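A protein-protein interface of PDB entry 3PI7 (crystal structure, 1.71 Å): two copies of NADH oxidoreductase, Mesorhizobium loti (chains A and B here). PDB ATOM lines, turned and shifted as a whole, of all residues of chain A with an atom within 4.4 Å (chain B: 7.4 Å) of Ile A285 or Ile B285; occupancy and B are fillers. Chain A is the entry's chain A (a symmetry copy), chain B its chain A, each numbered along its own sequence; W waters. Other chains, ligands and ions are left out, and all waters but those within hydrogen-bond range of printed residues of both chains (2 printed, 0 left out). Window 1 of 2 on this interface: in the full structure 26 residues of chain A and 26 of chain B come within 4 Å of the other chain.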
ATOM      1  N   PHE A 250      -6.002  31.030 -14.148  1.00  0.00           N
ATOM      2  CA  PHE A 250      -4.667  30.798 -14.654  1.00  0.00           C
ATOM      3  C   PHE A 250      -4.377  31.646 -15.887  1.00  0.00           C
ATOM      4  O   PHE A 250      -3.326  32.277 -15.975  1.00  0.00           O
ATOM      5  CB  PHE A 250      -4.514  29.321 -14.985  1.00  0.00           C
ATOM      6  CG  PHE A 250      -3.136  28.960 -15.481  1.00  0.00           C
ATOM      7  CD1 PHE A 250      -2.022  29.102 -14.654  1.00  0.00           C
ATOM      8  CD2 PHE A 250      -2.959  28.398 -16.748  1.00  0.00           C
ATOM      9  CE1 PHE A 250      -0.756  28.710 -15.086  1.00  0.00           C
ATOM     10  CE2 PHE A 250      -1.696  27.989 -17.175  1.00  0.00           C
ATOM     11  CZ  PHE A 250      -0.603  28.146 -16.339  1.00  0.00           C
ATOM     12  N   TRP A 259       0.190  27.354 -11.073  1.00  0.00           N
ATOM     13  CA  TRP A 259      -1.156  26.837 -10.798  1.00  0.00           C
ATOM     14  C   TRP A 259      -0.931  25.578 -10.014  1.00  0.00           C
ATOM     15  O   TRP A 259      -0.351  24.629 -10.549  1.00  0.00           O
ATOM     16  CB  TRP A 259      -1.841  26.584 -12.138  1.00  0.00           C
ATOM     17  CG  TRP A 259      -3.232  26.020 -12.131  1.00  0.00           C
ATOM     18  CD1 TRP A 259      -4.035  25.745 -11.059  1.00  0.00           C
ATOM     19  CD2 TRP A 259      -4.015  25.782 -13.299  1.00  0.00           C
ATOM     20  NE1 TRP A 259      -5.268  25.307 -11.498  1.00  0.00           N
ATOM     21  CE2 TRP A 259      -5.261  25.274 -12.874  1.00  0.00           C
ATOM     22  CE3 TRP A 259      -3.736  25.831 -14.682  1.00  0.00           C
ATOM     23  CZ2 TRP A 259      -6.264  24.911 -13.787  1.00  0.00           C
ATOM     24  CZ3 TRP A 259      -4.729  25.475 -15.584  1.00  0.00           C
ATOM     25  CH2 TRP A 259      -5.985  25.060 -15.140  1.00  0.00           C
ATOM     26  N   ILE A 261      -2.511  22.717  -8.021  1.00  0.00           N
ATOM     27  CA  ILE A 261      -3.793  22.021  -7.868  1.00  0.00           C
ATOM     28  C   ILE A 261      -3.716  21.118  -6.646  1.00  0.00           C
ATOM     29  O   ILE A 261      -2.815  20.287  -6.572  1.00  0.00           O
ATOM     30  CB  ILE A 261      -4.098  21.226  -9.166  1.00  0.00           C
ATOM     31  CG1 ILE A 261      -4.404  22.222 -10.310  1.00  0.00           C
ATOM     32  CG2 ILE A 261      -5.272  20.258  -8.920  1.00  0.00           C
ATOM     33  CD1 ILE A 261      -4.667  21.637 -11.739  1.00  0.00           C
ATOM     34  N   ILE A 272      -6.157  24.214 -20.453  1.00  0.00           N
ATOM     35  CA  ILE A 272      -5.061  25.201 -20.482  1.00  0.00           C
ATOM     36  C   ILE A 272      -5.458  26.061 -21.681  1.00  0.00           C
ATOM     37  O   ILE A 272      -5.226  25.673 -22.840  1.00  0.00           O
ATOM     38  CB  ILE A 272      -3.676  24.557 -20.621  1.00  0.00           C
ATOM     39  CG1 ILE A 272      -3.413  23.519 -19.510  1.00  0.00           C
ATOM     40  CG2 ILE A 272      -2.609  25.661 -20.637  1.00  0.00           C
ATOM     41  CD1 ILE A 272      -2.210  22.532 -19.803  1.00  0.00           C
ATOM     42  N   LEU A 278       2.637  29.113 -21.146  1.00  0.00           N
ATOM     43  CA  LEU A 278       3.671  28.345 -20.449  1.00  0.00           C
ATOM     44  C   LEU A 278       4.998  28.587 -21.157  1.00  0.00           C
ATOM     45  O   LEU A 278       6.034  28.648 -20.512  1.00  0.00           O
ATOM     46  CB  LEU A 278       3.344  26.854 -20.391  1.00  0.00           C
ATOM     47  CG  LEU A 278       2.172  26.509 -19.469  1.00  0.00           C
ATOM     48  CD1 LEU A 278       0.965  26.147 -20.282  1.00  0.00           C
ATOM     49  CD2 LEU A 278       2.533  25.419 -18.507  1.00  0.00           C
ATOM     50  N   HIS A 284       3.626  27.663 -14.880  1.00  0.00           N
ATOM     51  CA  HIS A 284       3.799  26.267 -14.493  1.00  0.00           C
ATOM     52  C   HIS A 284       2.519  25.738 -13.923  1.00  0.00           C
ATOM     53  O   HIS A 284       1.735  26.492 -13.346  1.00  0.00           O
ATOM     54  CB  HIS A 284       4.889  26.142 -13.407  1.00  0.00           C
ATOM     55  CG  HIS A 284       6.267  26.058 -13.937  1.00  0.00           C
ATOM     56  ND1 HIS A 284       6.959  27.200 -14.349  1.00  0.00           N
ATOM     57  CD2 HIS A 284       7.052  24.975 -14.123  1.00  0.00           C
ATOM     58  CE1 HIS A 284       8.136  26.770 -14.799  1.00  0.00           C
ATOM     59  NE2 HIS A 284       8.244  25.446 -14.689  1.00  0.00           N
ATOM     60  N   ILE A 285       2.319  24.450 -14.039  1.00  0.00           N
ATOM     61  CA  ILE A 285       1.149  23.794 -13.443  1.00  0.00           C
ATOM     62  C   ILE A 285       1.666  22.607 -12.659  1.00  0.00           C
ATOM     63  O   ILE A 285       2.390  21.779 -13.200  1.00  0.00           O
ATOM     64  CB  ILE A 285       0.062  23.358 -14.485  1.00  0.00           C
ATOM     65  CG1 ILE A 285      -0.226  24.488 -15.497  1.00  0.00           C
ATOM     66  CG2 ILE A 285      -1.243  22.867 -13.772  1.00  0.00           C
ATOM     67  CD1 ILE A 285      -1.161  24.115 -16.654  1.00  0.00           C
ATOM     68  N   GLU A 286       1.264  22.501 -11.393  1.00  0.00           N
ATOM     69  CA  GLU A 286       1.734  21.406 -10.556  1.00  0.00           C
ATOM     70  C   GLU A 286       0.626  20.986  -9.598  1.00  0.00           C
ATOM     71  O   GLU A 286      -0.452  21.577  -9.620  1.00  0.00           O
ATOM     72  CB  GLU A 286       2.975  21.856  -9.772  1.00  0.00           C
ATOM     73  CG  GLU A 286       2.729  23.115  -8.977  1.00  0.00           C
ATOM     74  CD  GLU A 286       3.971  23.780  -8.416  1.00  0.00           C
ATOM     75  OE1 GLU A 286       4.350  23.442  -7.271  1.00  0.00           O
ATOM     76  OE2 GLU A 286       4.527  24.676  -9.089  1.00  0.00           O
ATOM     77  N   PHE B 250       0.020  12.798 -21.940  1.00  0.00           N
ATOM     78  CA  PHE B 250       0.234  13.168 -20.558  1.00  0.00           C
ATOM     79  C   PHE B 250      -0.554  12.275 -19.608  1.00  0.00           C
ATOM     80  O   PHE B 250      -0.012  11.786 -18.619  1.00  0.00           O
ATOM     81  CB  PHE B 250      -0.167  14.623 -20.368  1.00  0.00           C
ATOM     82  CG  PHE B 250       0.061  15.126 -18.964  1.00  0.00           C
ATOM     83  CD1 PHE B 250       1.349  15.197 -18.434  1.00  0.00           C
ATOM     84  CD2 PHE B 250      -1.003  15.609 -18.199  1.00  0.00           C
ATOM     85  CE1 PHE B 250       1.570  15.721 -17.162  1.00  0.00           C
ATOM     86  CE2 PHE B 250      -0.781  16.150 -16.933  1.00  0.00           C
ATOM     87  CZ  PHE B 250       0.506  16.205 -16.425  1.00  0.00           C
ATOM     88  N   ALA B 257       5.745  12.556 -14.296  1.00  0.00           N
ATOM     89  CA  ALA B 257       5.852  13.008 -15.665  1.00  0.00           C
ATOM     90  C   ALA B 257       5.831  14.516 -15.749  1.00  0.00           C
ATOM     91  O   ALA B 257       5.123  15.174 -14.985  1.00  0.00           O
ATOM     92  CB  ALA B 257       4.727  12.452 -16.489  1.00  0.00           C
ATOM     93  N   ARG B 258       6.667  15.048 -16.648  1.00  0.00           N
ATOM     94  CA  ARG B 258       6.760  16.491 -16.914  1.00  0.00           C
ATOM     95  C   ARG B 258       6.350  16.728 -18.362  1.00  0.00           C
ATOM     96  O   ARG B 258       6.975  16.187 -19.300  1.00  0.00           O
ATOM     97  CB  ARG B 258       8.181  17.000 -16.674  1.00  0.00           C
ATOM     98  CG  ARG B 258       8.592  16.972 -15.209  1.00  0.00           C
ATOM     99  CD  ARG B 258      10.072  17.219 -15.084  1.00  0.00           C
ATOM    100  NE  ARG B 258      10.474  18.522 -15.602  1.00  0.00           N
ATOM    101  CZ  ARG B 258      11.742  18.867 -15.821  1.00  0.00           C
ATOM    102  NH1 ARG B 258      12.722  18.001 -15.594  1.00  0.00           N
ATOM    103  NH2 ARG B 258      12.037  20.074 -16.281  1.00  0.00           N
ATOM    104  N   TRP B 259       5.285  17.492 -18.542  1.00  0.00           N
ATOM    105  CA  TRP B 259       4.768  17.843 -19.870  1.00  0.00           C
ATOM    106  C   TRP B 259       5.382  19.177 -20.180  1.00  0.00           C
ATOM    107  O   TRP B 259       5.092  20.151 -19.481  1.00  0.00           O
ATOM    108  CB  TRP B 259       3.246  17.900 -19.776  1.00  0.00           C
ATOM    109  CG  TRP B 259       2.471  18.271 -21.007  1.00  0.00           C
ATOM    110  CD1 TRP B 259       2.940  18.517 -22.269  1.00  0.00           C
ATOM    111  CD2 TRP B 259       1.048  18.314 -21.086  1.00  0.00           C
ATOM    112  NE1 TRP B 259       1.882  18.752 -23.124  1.00  0.00           N
ATOM    113  CE2 TRP B 259       0.710  18.681 -22.406  1.00  0.00           C
ATOM    114  CE3 TRP B 259       0.018  18.198 -20.127  1.00  0.00           C
ATOM    115  CZ2 TRP B 259      -0.625  18.836 -22.814  1.00  0.00           C
ATOM    116  CZ3 TRP B 259      -1.301  18.348 -20.531  1.00  0.00           C
ATOM    117  CH2 TRP B 259      -1.616  18.624 -21.862  1.00  0.00           C
ATOM    118  N   ILE B 260       6.348  19.179 -21.100  1.00  0.00           N
ATOM    119  CA  ILE B 260       7.122  20.375 -21.442  1.00  0.00           C
ATOM    120  C   ILE B 260       6.669  20.873 -22.797  1.00  0.00           C
ATOM    121  O   ILE B 260       6.940  20.258 -23.820  1.00  0.00           O
ATOM    122  CB  ILE B 260       8.637  20.097 -21.403  1.00  0.00           C
ATOM    123  CG1 ILE B 260       9.035  19.550 -20.018  1.00  0.00           C
ATOM    124  CG2 ILE B 260       9.413  21.400 -21.761  1.00  0.00           C
ATOM    125  CD1 ILE B 260      10.495  19.174 -19.831  1.00  0.00           C
ATOM    126  N   ILE B 261       5.894  21.942 -22.776  1.00  0.00           N
ATOM    127  CA  ILE B 261       5.281  22.470 -24.000  1.00  0.00           C
ATOM    128  C   ILE B 261       6.240  23.466 -24.636  1.00  0.00           C
ATOM    129  O   ILE B 261       6.648  24.413 -23.971  1.00  0.00           O
ATOM    130  CB  ILE B 261       3.915  23.117 -23.646  1.00  0.00           C
ATOM    131  CG1 ILE B 261       2.919  22.005 -23.237  1.00  0.00           C
ATOM    132  CG2 ILE B 261       3.400  23.935 -24.846  1.00  0.00           C
ATOM    133  CD1 ILE B 261       1.491  22.440 -22.764  1.00  0.00           C
ATOM    134  N   THR B 270      -6.575  22.194 -25.114  1.00  0.00           N
ATOM    135  CA  THR B 270      -5.623  21.354 -24.389  1.00  0.00           C
ATOM    136  C   THR B 270      -6.210  21.109 -23.006  1.00  0.00           C
ATOM    137  O   THR B 270      -6.327  22.034 -22.194  1.00  0.00           O
ATOM    138  CB  THR B 270      -4.238  21.970 -24.347  1.00  0.00           C
ATOM    139  OG1 THR B 270      -3.789  22.181 -25.673  1.00  0.00           O
ATOM    140  CG2 THR B 270      -3.238  21.098 -23.626  1.00  0.00           C
ATOM    141  N   VAL B 271      -6.590  19.868 -22.760  1.00  0.00           N
ATOM    142  CA  VAL B 271      -7.265  19.488 -21.520  1.00  0.00           C
ATOM    143  C   VAL B 271      -6.310  18.738 -20.612  1.00  0.00           C
ATOM    144  O   VAL B 271      -5.558  17.894 -21.082  1.00  0.00           O
ATOM    145  CB  VAL B 271      -8.535  18.634 -21.826  1.00  0.00           C
ATOM    146  CG1 VAL B 271      -9.154  18.046 -20.558  1.00  0.00           C
ATOM    147  CG2 VAL B 271      -9.580  19.435 -22.601  1.00  0.00           C
ATOM    148  N   ILE B 272      -6.340  19.035 -19.316  1.00  0.00           N
ATOM    149  CA  ILE B 272      -5.676  18.205 -18.293  1.00  0.00           C
ATOM    150  C   ILE B 272      -6.783  17.210 -17.944  1.00  0.00           C
ATOM    151  O   ILE B 272      -7.705  17.538 -17.174  1.00  0.00           O
ATOM    152  CB  ILE B 272      -5.179  19.015 -17.090  1.00  0.00           C
ATOM    153  CG1 ILE B 272      -4.239  20.161 -17.521  1.00  0.00           C
ATOM    154  CG2 ILE B 272      -4.504  18.067 -16.090  1.00  0.00           C
ATOM    155  CD1 ILE B 272      -4.010  21.275 -16.419  1.00  0.00           C
ATOM    156  N   LEU B 278      -1.815  15.319 -11.097  1.00  0.00           N
ATOM    157  CA  LEU B 278      -0.799  16.269 -10.638  1.00  0.00           C
ATOM    158  C   LEU B 278      -0.698  16.154  -9.122  1.00  0.00           C
ATOM    159  O   LEU B 278       0.386  16.282  -8.570  1.00  0.00           O
ATOM    160  CB  LEU B 278      -1.115  17.703 -11.059  1.00  0.00           C
ATOM    161  CG  LEU B 278      -0.971  17.956 -12.561  1.00  0.00           C
ATOM    162  CD1 LEU B 278      -2.323  18.092 -13.194  1.00  0.00           C
ATOM    163  CD2 LEU B 278      -0.115  19.155 -12.835  1.00  0.00           C
ATOM    164  N   HIS B 282       2.221  13.339  -8.884  1.00  0.00           N
ATOM    165  CA  HIS B 282       3.286  14.354  -8.880  1.00  0.00           C
ATOM    166  C   HIS B 282       3.674  14.831 -10.282  1.00  0.00           C
ATOM    167  O   HIS B 282       4.848  15.138 -10.533  1.00  0.00           O
ATOM    168  CB  HIS B 282       4.543  13.801  -8.150  1.00  0.00           C
ATOM    169  CG  HIS B 282       4.226  12.780  -7.084  1.00  0.00           C
ATOM    170  ND1 HIS B 282       3.517  13.122  -5.933  1.00  0.00           N
ATOM    171  CD2 HIS B 282       4.456  11.441  -7.073  1.00  0.00           C
ATOM    172  CE1 HIS B 282       3.369  11.996  -5.251  1.00  0.00           C
ATOM    173  NE2 HIS B 282       3.941  10.956  -5.886  1.00  0.00           N
ATOM    174  N   LYS B 283       2.704  14.887 -11.191  1.00  0.00           N
ATOM    175  CA  LYS B 283       2.968  15.314 -12.576  1.00  0.00           C
ATOM    176  C   LYS B 283       3.073  16.837 -12.628  1.00  0.00           C
ATOM    177  O   LYS B 283       2.557  17.519 -11.739  1.00  0.00           O
ATOM    178  CB  LYS B 283       1.883  14.806 -13.547  1.00  0.00           C
ATOM    179  CG  LYS B 283       1.899  13.294 -13.735  1.00  0.00           C
ATOM    180  CD  LYS B 283       0.956  12.873 -14.853  1.00  0.00           C
ATOM    181  CE  LYS B 283       0.980  11.363 -14.959  1.00  0.00           C
ATOM    182  NZ  LYS B 283       0.007  10.890 -16.015  1.00  0.00           N
ATOM    183  N   HIS B 284       3.828  17.358 -13.617  1.00  0.00           N
ATOM    184  CA  HIS B 284       4.059  18.790 -13.777  1.00  0.00           C
ATOM    185  C   HIS B 284       3.824  19.185 -15.202  1.00  0.00           C
ATOM    186  O   HIS B 284       4.019  18.378 -16.113  1.00  0.00           O
ATOM    187  CB  HIS B 284       5.519  19.141 -13.421  1.00  0.00           C
ATOM    188  CG  HIS B 284       5.755  19.369 -11.979  1.00  0.00           C
ATOM    189  ND1 HIS B 284       5.908  18.302 -11.090  1.00  0.00           N
ATOM    190  CD2 HIS B 284       5.850  20.530 -11.296  1.00  0.00           C
ATOM    191  CE1 HIS B 284       6.064  18.850  -9.887  1.00  0.00           C
ATOM    192  NE2 HIS B 284       6.035  20.182  -9.952  1.00  0.00           N
ATOM    193  N   ILE B 285       3.451  20.422 -15.410  1.00  0.00           N
ATOM    194  CA  ILE B 285       3.278  20.958 -16.765  1.00  0.00           C
ATOM    195  C   ILE B 285       4.049  22.260 -16.821  1.00  0.00           C
ATOM    196  O   ILE B 285       3.844  23.134 -15.986  1.00  0.00           O
ATOM    197  CB  ILE B 285       1.781  21.165 -17.182  1.00  0.00           C
ATOM    198  CG1 ILE B 285       0.924  19.933 -16.817  1.00  0.00           C
ATOM    199  CG2 ILE B 285       1.661  21.529 -18.700  1.00  0.00           C
ATOM    200  CD1 ILE B 285      -0.585  20.089 -17.040  1.00  0.00           C
ATOM    201  N   GLU B 286       4.908  22.406 -17.828  1.00  0.00           N
ATOM    202  CA  GLU B 286       5.712  23.615 -17.946  1.00  0.00           C
ATOM    203  C   GLU B 286       5.910  23.953 -19.418  1.00  0.00           C
ATOM    204  O   GLU B 286       5.424  23.224 -20.280  1.00  0.00           O
ATOM    205  CB  GLU B 286       7.069  23.396 -17.261  1.00  0.00           C
ATOM    206  CG  GLU B 286       7.790  22.179 -17.789  1.00  0.00           C
ATOM    207  CD  GLU B 286       8.987  21.730 -16.972  1.00  0.00           C
ATOM    208  OE1 GLU B 286      10.108  22.201 -17.269  1.00  0.00           O
ATOM    209  OE2 GLU B 286       8.815  20.869 -16.081  1.00  0.00           O
ATOM    210  N   GLY B 287       6.634  25.039 -19.673  1.00  0.00           N
ATOM    211  CA  GLY B 287       6.964  25.424 -21.033  1.00  0.00           C
ATOM    212  C   GLY B 287       8.463  25.490 -21.230  1.00  0.00           C
ATOM    213  O   GLY B 287       9.235  25.529 -20.271  1.00  0.00           O
HETATM  214  O   HOH W   1      -6.274  24.933 -25.145  1.00  0.00           O
HETATM  215  O   HOH W   2       7.050  27.325 -18.018  1.00  0.00           O
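The backbone NH (N) of Ile A272 lies within hydrogen-bond range of the backbone carbonyl oxygen (O) of Thr B270 (2.8 Å).
The backbone NH (N) of Ile B285 sits at hydrogen-bond distance from the backbone carbonyl oxygen (O) of Ile A285 (2.8 Å).
The backbone NH of Ile A261 sits at hydrogen-bond distance from the backbone carbonyl oxygen of Glu A286, 2.8 Å away.
The backbone NH of Glu B286 sits at hydrogen-bond distance from the backbone carbonyl oxygen of Trp B259 (2.8 Å).
The backbone carbonyl oxygen (O) of Ala B257 is in hydrogen-bond range of the backbone NH (N) of His B284, at 2.9 Å.
N of Glu A286 sits at hydrogen-bond distance from O of Trp A259 (2.8 Å).
The backbone carbonyl oxygen of His B282 is in hydrogen-bond range of a ring nitrogen (ND1) of His B284.
OE2 of Glu B286 lies within salt-bridge range of NE of Arg B258 (2.9 Å).
Ile A272 touches Ile B272.
Leu A278 touches Ile B285 (CD2 to O, 3.6 Å).
CD2 of Leu A278 touches CA of Glu B286, at 3.7 Å.
Gly B287 touches Leu A278 (CA to O, 3.4 Å).
His A284 touches Ile B285 (CA to O, 3.5 Å).
His A284 touches Glu B286 (NE2 to CB, 3.5 Å).
CD2 of Leu B278 touches O of Ile A285 (3.6 Å).
O of Ile A285 touches CA of His B284, 3.5 Å away.
Glu A286 touches Leu B278.
His B284 touches Glu A286 (NE2 to CB, 3.5 Å).
Ile A261 touches none of the printed residues of chain B.
Of the printed residues of chain B, Ile A285 touches Leu B278 (3.6 Å), His B284 (3.5 Å) and Ile B285 (2.8 Å).
Printed residues of chain A within 4 Å of Ile B285: Leu A278 (3.6 Å), His A284 (3.5 Å) and Ile A285 (2.8 Å).
Of the printed residues of chain A, Glu B286 touches Leu A278 and His A284.
Printed residues of chain A within 4 Å of Gly B287: Leu A278.
The nearest printed residue of chain B that does not touch Ile A285 is Ile B272 (4.03 Å).
The nearest printed residue of chain A that does not touch His B284 is His A284 (5.4 Å).
Of the 8 printed residues of chain A, 5 touch a printed residue of chain B.
Printed residues of chain A that touch a printed residue of chain B: Ile A272, Leu A278, His A284, Ile A285 and Glu A286.
Hydrophobic or aromatic side chains of chain A that line the printed part of chain B: Ile A272, Leu A278, His A284 and Ile A285.
Of the 16 printed residues of chain B, 7 touch a printed residue of chain A.
Printed residues of chain B that touch a printed residue of chain A: Thr B270, Ile B272, Leu B278, His B284, Ile B285, Glu B286 and Gly B287.
Hydrophobic or aromatic side chains of chain B within 4 Å of the printed part of chain A: Ile B272, Leu B278, His B284 and Ile B285.
Among the printed residues, no Asp or Glu carboxylate lies within 4 Å of a Lys or Arg side-chain nitrogen of the other chain.
Ile A272 touches its own counterpart, Ile B272.
Leu A278 touches Ile B285, and with the chains exchanged Ile A285 touches Leu B278.
Leu A278 touches Glu B286, and with the chains exchanged Glu A286 touches Leu B278.
His A284 touches Glu B286, and with the chains exchanged Glu A286 touches His B284.
Water W1 lies within hydrogen-bond range of O of Ile A272 (2.6 Å) and N of Thr B270 (2.8 Å).
Water W2 lies within hydrogen-bond range of N of Gly B287 and O of Leu A278.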
